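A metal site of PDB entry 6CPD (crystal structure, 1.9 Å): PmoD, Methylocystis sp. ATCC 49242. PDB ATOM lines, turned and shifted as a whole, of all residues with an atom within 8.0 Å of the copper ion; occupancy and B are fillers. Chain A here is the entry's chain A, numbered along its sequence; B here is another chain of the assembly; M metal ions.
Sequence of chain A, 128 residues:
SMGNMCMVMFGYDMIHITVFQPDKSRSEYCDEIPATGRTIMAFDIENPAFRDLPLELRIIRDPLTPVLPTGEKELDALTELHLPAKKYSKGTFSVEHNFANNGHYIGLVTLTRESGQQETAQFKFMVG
O of Met 5 of chain A is in hydrogen-bond range of N of Met 7 of chain B (2.9 Å). N of Met 7 of chain A lies within hydrogen-bond range of O of Met 5 of chain B (3.0 Å).
SD of Met 9 of chain B is bound to the copper ion, 2.3 Å away. SD of Met 7 of chain B is bound to the copper ion, 2.3 Å away. The copper ion is bound by the side-chain sulfur (SD) of Met 7 of chain A (2.3 Å). SD of Met 9 of chain A is bound to the copper ion (2.4 Å).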
ATOM      1  N   ASN A   4       3.886   0.265  19.540  1.00  0.00           N
ATOM      2  CA  ASN A   4       3.284   0.813  18.342  1.00  0.00           C
ATOM      3  C   ASN A   4       3.893   2.182  18.045  1.00  0.00           C
ATOM      4  O   ASN A   4       3.714   2.760  16.968  1.00  0.00           O
ATOM      5  CB  ASN A   4       1.763   0.915  18.500  1.00  0.00           C
ATOM      6  CG  ASN A   4       1.178   2.090  17.752  1.00  0.00           C
ATOM      7  OD1 ASN A   4       1.092   3.200  18.293  1.00  0.00           O
ATOM      8  ND2 ASN A   4       0.836   1.880  16.485  1.00  0.00           N
ATOM      9  N   MET A   5       4.656   2.705  18.999  1.00  0.00           N
ATOM     10  CA  MET A   5       5.136   4.066  18.799  1.00  0.00           C
ATOM     11  C   MET A   5       6.629   4.114  18.496  1.00  0.00           C
ATOM     12  O   MET A   5       7.108   5.074  17.931  1.00  0.00           O
ATOM     13  CB  MET A   5       4.836   4.956  20.013  1.00  0.00           C
ATOM     14  CG  MET A   5       3.383   5.221  20.282  1.00  0.00           C
ATOM     15  SD  MET A   5       3.111   6.034  21.901  1.00  0.00           S
ATOM     16  CE  MET A   5       3.934   7.605  21.637  1.00  0.00           C
ATOM     17  N   CYS A   6       7.374   3.095  18.923  1.00  0.00           N
ATOM     18  CA  CYS A   6       8.833   3.119  18.795  1.00  0.00           C
ATOM     19  C   CYS A   6       9.311   2.295  17.590  1.00  0.00           C
ATOM     20  O   CYS A   6       9.069   1.076  17.545  1.00  0.00           O
ATOM     21  CB  CYS A   6       9.476   2.588  20.087  1.00  0.00           C
ATOM     22  SG  CYS A   6      11.287   2.757  20.091  1.00  0.00           S
ATOM     23  N   MET A   7       9.946   2.942  16.617  1.00  0.00           N
ATOM     24  CA  MET A   7      10.222   2.265  15.362  1.00  0.00           C
ATOM     25  C   MET A   7      11.316   2.964  14.552  1.00  0.00           C
ATOM     26  O   MET A   7      11.636   4.131  14.788  1.00  0.00           O
ATOM     27  CB  MET A   7       8.954   2.178  14.541  1.00  0.00           C
ATOM     28  CG  MET A   7       8.491   3.555  14.061  1.00  0.00           C
ATOM     29  SD  MET A   7       6.829   3.456  13.402  1.00  0.00           S
ATOM     30  CE  MET A   7       5.861   3.410  14.915  1.00  0.00           C
ATOM     31  N   VAL A   8      11.846   2.238  13.577  1.00  0.00           N
ATOM     32  CA  VAL A   8      12.592   2.840  12.476  1.00  0.00           C
ATOM     33  C   VAL A   8      11.786   2.632  11.185  1.00  0.00           C
ATOM     34  O   VAL A   8      11.166   1.586  11.002  1.00  0.00           O
ATOM     35  CB  VAL A   8      14.025   2.252  12.362  1.00  0.00           C
ATOM     36  CG1 VAL A   8      13.987   0.746  12.142  1.00  0.00           C
ATOM     37  CG2 VAL A   8      14.845   2.973  11.266  1.00  0.00           C
ATOM     38  N   MET A   9      11.799   3.625  10.285  1.00  0.00           N
ATOM     39  CA  MET A   9      10.912   3.638   9.109  1.00  0.00           C
ATOM     40  C   MET A   9      11.682   3.330   7.844  1.00  0.00           C
ATOM     41  O   MET A   9      12.817   3.761   7.683  1.00  0.00           O
ATOM     42  CB  MET A   9      10.234   5.011   8.903  1.00  0.00           C
ATOM     43  CG  MET A   9       9.457   5.570  10.070  1.00  0.00           C
ATOM     44  SD  MET A   9       8.084   4.501  10.418  1.00  0.00           S
ATOM     45  CE  MET A   9       7.136   4.548   8.879  1.00  0.00           C
ATOM     46  N   PHE A  10      11.061   2.550   6.963  1.00  0.00           N
ATOM     47  CA  PHE A  10      11.489   2.394   5.576  1.00  0.00           C
ATOM     48  C   PHE A  10      10.308   2.843   4.718  1.00  0.00           C
ATOM     49  O   PHE A  10       9.465   2.027   4.351  1.00  0.00           O
ATOM     50  CB  PHE A  10      11.866   0.944   5.255  1.00  0.00           C
ATOM     51  CG  PHE A  10      13.148   0.485   5.917  1.00  0.00           C
ATOM     52  CD1 PHE A  10      13.156   0.037   7.223  1.00  0.00           C
ATOM     53  CD2 PHE A  10      14.345   0.460   5.206  1.00  0.00           C
ATOM     54  CE1 PHE A  10      14.340  -0.394   7.832  1.00  0.00           C
ATOM     55  CE2 PHE A  10      15.534   0.031   5.791  1.00  0.00           C
ATOM     56  CZ  PHE A  10      15.529  -0.397   7.116  1.00  0.00           C
ATOM     57  N   GLY A  11      10.233   4.129   4.424  1.00  0.00           N
ATOM     58  CA  GLY A  11       9.074   4.655   3.729  1.00  0.00           C
ATOM     59  C   GLY A  11       7.888   4.548   4.671  1.00  0.00           C
ATOM     60  O   GLY A  11       7.928   5.096   5.767  1.00  0.00           O
ATOM     61  N   TYR A  12       6.837   3.837   4.250  1.00  0.00           N
ATOM     62  CA  TYR A  12       5.659   3.609   5.087  1.00  0.00           C
ATOM     63  C   TYR A  12       5.837   2.388   5.989  1.00  0.00           C
ATOM     64  O   TYR A  12       5.031   2.171   6.900  1.00  0.00           O
ATOM     65  CB  TYR A  12       4.409   3.416   4.234  1.00  0.00           C
ATOM     66  CG  TYR A  12       3.991   4.619   3.442  1.00  0.00           C
ATOM     67  CD1 TYR A  12       3.836   5.859   4.049  1.00  0.00           C
ATOM     68  CD2 TYR A  12       3.775   4.524   2.070  1.00  0.00           C
ATOM     69  CE1 TYR A  12       3.456   6.976   3.306  1.00  0.00           C
ATOM     70  CE2 TYR A  12       3.399   5.620   1.323  1.00  0.00           C
ATOM     71  CZ  TYR A  12       3.245   6.851   1.950  1.00  0.00           C
ATOM     72  OH  TYR A  12       2.871   7.940   1.191  1.00  0.00           O
ATOM     73  N   ASP A  13       6.847   1.560   5.685  1.00  0.00           N
ATOM     74  CA  ASP A  13       7.098   0.308   6.421  1.00  0.00           C
ATOM     75  C   ASP A  13       7.890   0.555   7.690  1.00  0.00           C
ATOM     76  O   ASP A  13       8.647   1.523   7.773  1.00  0.00           O
ATOM     77  CB  ASP A  13       7.825  -0.724   5.545  1.00  0.00           C
ATOM     78  CG  ASP A  13       6.967  -1.215   4.384  1.00  0.00           C
ATOM     79  OD1 ASP A  13       5.951  -1.896   4.651  1.00  0.00           O
ATOM     80  OD2 ASP A  13       7.304  -0.920   3.209  1.00  0.00           O
ATOM     81  N   MET A  14       7.611  -0.235   8.726  1.00  0.00           N
ATOM     82  CA  MET A  14       8.277  -0.054  10.018  1.00  0.00           C
ATOM     83  C   MET A  14       8.928  -1.322  10.574  1.00  0.00           C
ATOM     84  O   MET A  14       8.467  -2.445  10.327  1.00  0.00           O
ATOM     85  CB  MET A  14       7.267   0.464  11.026  1.00  0.00           C
ATOM     86  CG  MET A  14       6.062  -0.457  11.147  1.00  0.00           C
ATOM     87  SD  MET A  14       4.589   0.425  11.674  1.00  0.00           S
ATOM     88  CE  MET A  14       4.452   1.549  10.307  1.00  0.00           C
ATOM     89  N   ILE A  15       9.968  -1.115  11.364  1.00  0.00           N
ATOM     90  CA  ILE A  15      10.483  -2.159  12.266  1.00  0.00           C
ATOM     91  C   ILE A  15      10.316  -1.597  13.669  1.00  0.00           C
ATOM     92  O   ILE A  15      10.874  -0.556  13.997  1.00  0.00           O
ATOM     93  CB  ILE A  15      11.947  -2.502  11.983  1.00  0.00           C
ATOM     94  CG1 ILE A  15      12.092  -3.031  10.560  1.00  0.00           C
ATOM     95  CG2 ILE A  15      12.449  -3.530  12.979  1.00  0.00           C
ATOM     96  CD1 ILE A  15      13.541  -3.330  10.179  1.00  0.00           C
ATOM     97  N   HIS A  16       9.528  -2.275  14.506  1.00  0.00           N
ATOM     98  CA  HIS A  16       9.339  -1.765  15.868  1.00  0.00           C
ATOM     99  C   HIS A  16      10.525  -2.151  16.743  1.00  0.00           C
ATOM    100  O   HIS A  16      11.128  -3.231  16.579  1.00  0.00           O
ATOM    101  CB  HIS A  16       8.028  -2.252  16.456  1.00  0.00           C
ATOM    102  CG  HIS A  16       6.824  -1.875  15.631  1.00  0.00           C
ATOM    103  ND1 HIS A  16       6.218  -0.647  15.727  1.00  0.00           N
ATOM    104  CD2 HIS A  16       6.161  -2.559  14.670  1.00  0.00           C
ATOM    105  CE1 HIS A  16       5.212  -0.589  14.879  1.00  0.00           C
ATOM    106  NE2 HIS A  16       5.153  -1.731  14.221  1.00  0.00           N
ATOM    107  N   ASN B   4      14.788  10.008  16.991  1.00  0.00           N
ATOM    108  CA  ASN B   4      13.756   9.990  15.969  1.00  0.00           C
ATOM    109  C   ASN B   4      12.830   8.783  15.983  1.00  0.00           C
ATOM    110  O   ASN B   4      12.184   8.494  14.975  1.00  0.00           O
ATOM    111  CB  ASN B   4      14.398  10.118  14.582  1.00  0.00           C
ATOM    112  CG  ASN B   4      15.107   8.861  14.155  1.00  0.00           C
ATOM    113  OD1 ASN B   4      15.354   7.946  14.967  1.00  0.00           O
ATOM    114  ND2 ASN B   4      15.464   8.791  12.874  1.00  0.00           N
ATOM    115  N   MET B   5      12.771   8.036  17.095  1.00  0.00           N
ATOM    116  CA  MET B   5      12.145   6.717  17.035  1.00  0.00           C
ATOM    117  C   MET B   5      10.720   6.659  17.570  1.00  0.00           C
ATOM    118  O   MET B   5       9.912   5.861  17.103  1.00  0.00           O
ATOM    119  CB  MET B   5      12.999   5.717  17.822  1.00  0.00           C
ATOM    120  CG  MET B   5      14.386   5.526  17.241  1.00  0.00           C
ATOM    121  SD  MET B   5      15.492   4.724  18.437  1.00  0.00           S
ATOM    122  CE  MET B   5      14.608   3.182  18.589  1.00  0.00           C
ATOM    123  N   CYS B   6      10.391   7.545  18.501  1.00  0.00           N
ATOM    124  CA  CYS B   6       9.083   7.516  19.144  1.00  0.00           C
ATOM    125  C   CYS B   6       8.157   8.497  18.428  1.00  0.00           C
ATOM    126  O   CYS B   6       8.402   9.680  18.468  1.00  0.00           O
ATOM    127  CB  CYS B   6       9.208   7.890  20.631  1.00  0.00           C
ATOM    128  SG  CYS B   6       7.617   7.894  21.526  1.00  0.00           S
ATOM    129  N   MET B   7       7.085   8.011  17.792  1.00  0.00           N
ATOM    130  CA  MET B   7       6.355   8.913  16.898  1.00  0.00           C
ATOM    131  C   MET B   7       4.890   8.593  16.720  1.00  0.00           C
ATOM    132  O   MET B   7       4.460   7.474  16.940  1.00  0.00           O
ATOM    133  CB  MET B   7       6.997   8.885  15.502  1.00  0.00           C
ATOM    134  CG  MET B   7       6.828   7.515  14.808  1.00  0.00           C
ATOM    135  SD  MET B   7       7.694   7.298  13.231  1.00  0.00           S
ATOM    136  CE  MET B   7       9.403   7.183  13.821  1.00  0.00           C
ATOM    137  N   VAL B   8       4.141   9.592  16.270  1.00  0.00           N
ATOM    138  CA  VAL B   8       2.818   9.372  15.685  1.00  0.00           C
ATOM    139  C   VAL B   8       2.933   9.792  14.204  1.00  0.00           C
ATOM    140  O   VAL B   8       3.712  10.673  13.886  1.00  0.00           O
ATOM    141  CB  VAL B   8       1.725  10.154  16.433  1.00  0.00           C
ATOM    142  CG1 VAL B   8       1.972  11.639  16.334  1.00  0.00           C
ATOM    143  CG2 VAL B   8       0.370   9.790  15.909  1.00  0.00           C
ATOM    144  N   MET B   9       2.262   9.091  13.299  1.00  0.00           N
ATOM    145  CA  MET B   9       2.527   9.270  11.868  1.00  0.00           C
ATOM    146  C   MET B   9       1.368   9.773  11.017  1.00  0.00           C
ATOM    147  O   MET B   9       0.247   9.299  11.146  1.00  0.00           O
ATOM    148  CB  MET B   9       3.008   7.942  11.299  1.00  0.00           C
ATOM    149  CG  MET B   9       4.195   7.369  12.086  1.00  0.00           C
ATOM    150  SD  MET B   9       4.764   5.875  11.319  1.00  0.00           S
ATOM    151  CE  MET B   9       3.476   4.729  11.807  1.00  0.00           C
ATOM    152  N   PHE B  10       1.676  10.694  10.094  1.00  0.00           N
ATOM    153  CA  PHE B  10       0.760  11.031   9.013  1.00  0.00           C
ATOM    154  C   PHE B  10       1.466  10.790   7.696  1.00  0.00           C
ATOM    155  O   PHE B  10       2.046  11.718   7.139  1.00  0.00           O
ATOM    156  CB  PHE B  10       0.308  12.493   9.084  1.00  0.00           C
ATOM    157  CG  PHE B  10      -0.526  12.806  10.288  1.00  0.00           C
ATOM    158  CD1 PHE B  10       0.068  13.115  11.495  1.00  0.00           C
ATOM    159  CD2 PHE B  10      -1.911  12.769  10.209  1.00  0.00           C
ATOM    160  CE1 PHE B  10      -0.699  13.405  12.625  1.00  0.00           C
ATOM    161  CE2 PHE B  10      -2.693  13.055  11.324  1.00  0.00           C
ATOM    162  CZ  PHE B  10      -2.092  13.370  12.528  1.00  0.00           C
ATOM    163  N   GLY B  11       1.409   9.572   7.181  1.00  0.00           N
ATOM    164  CA  GLY B  11       2.138   9.264   5.966  1.00  0.00           C
ATOM    165  C   GLY B  11       3.620   9.369   6.241  1.00  0.00           C
ATOM    166  O   GLY B  11       4.142   8.697   7.131  1.00  0.00           O
ATOM    167  N   TYR B  12       4.329  10.218   5.512  1.00  0.00           N
ATOM    168  CA  TYR B  12       5.748  10.402   5.770  1.00  0.00           C
ATOM    169  C   TYR B  12       5.991  11.427   6.860  1.00  0.00           C
ATOM    170  O   TYR B  12       7.105  11.570   7.349  1.00  0.00           O
ATOM    171  CB  TYR B  12       6.491  10.845   4.508  1.00  0.00           C
ATOM    172  CG  TYR B  12       6.464   9.847   3.396  1.00  0.00           C
ATOM    173  CD1 TYR B  12       6.855   8.520   3.607  1.00  0.00           C
ATOM    174  CD2 TYR B  12       6.020  10.211   2.131  1.00  0.00           C
ATOM    175  CE1 TYR B  12       6.834   7.602   2.567  1.00  0.00           C
ATOM    176  CE2 TYR B  12       5.988   9.308   1.098  1.00  0.00           C
ATOM    177  CZ  TYR B  12       6.391   8.000   1.317  1.00  0.00           C
ATOM    178  OH  TYR B  12       6.354   7.128   0.268  1.00  0.00           O
ATOM    179  N   ASP B  13       4.960  12.206   7.178  1.00  0.00           N
ATOM    180  CA  ASP B  13       5.153  13.276   8.143  1.00  0.00           C
ATOM    181  C   ASP B  13       4.943  12.736   9.551  1.00  0.00           C
ATOM    182  O   ASP B  13       3.867  12.229   9.864  1.00  0.00           O
ATOM    183  CB  ASP B  13       4.201  14.428   7.840  1.00  0.00           C
ATOM    184  CG  ASP B  13       4.322  14.916   6.397  1.00  0.00           C
ATOM    185  OD1 ASP B  13       5.402  15.407   6.005  1.00  0.00           O
ATOM    186  OD2 ASP B  13       3.318  14.794   5.658  1.00  0.00           O
ATOM    187  N   MET B  14       5.916  12.956  10.435  1.00  0.00           N
ATOM    188  CA  MET B  14       5.875  12.361  11.777  1.00  0.00           C
ATOM    189  C   MET B  14       5.823  13.473  12.794  1.00  0.00           C
ATOM    190  O   MET B  14       6.215  14.615  12.517  1.00  0.00           O
ATOM    191  CB  MET B  14       7.093  11.459  12.064  1.00  0.00           C
ATOM    192  CG  MET B  14       7.464  10.468  10.960  1.00  0.00           C
ATOM    193  SD  MET B  14       6.008   9.650  10.260  1.00  0.00           S
ATOM    194  CE  MET B  14       6.774   8.343   9.291  1.00  0.00           C
HETATM  195 CU    CU M   1       6.810   5.436  12.231  1.00  0.00          CU
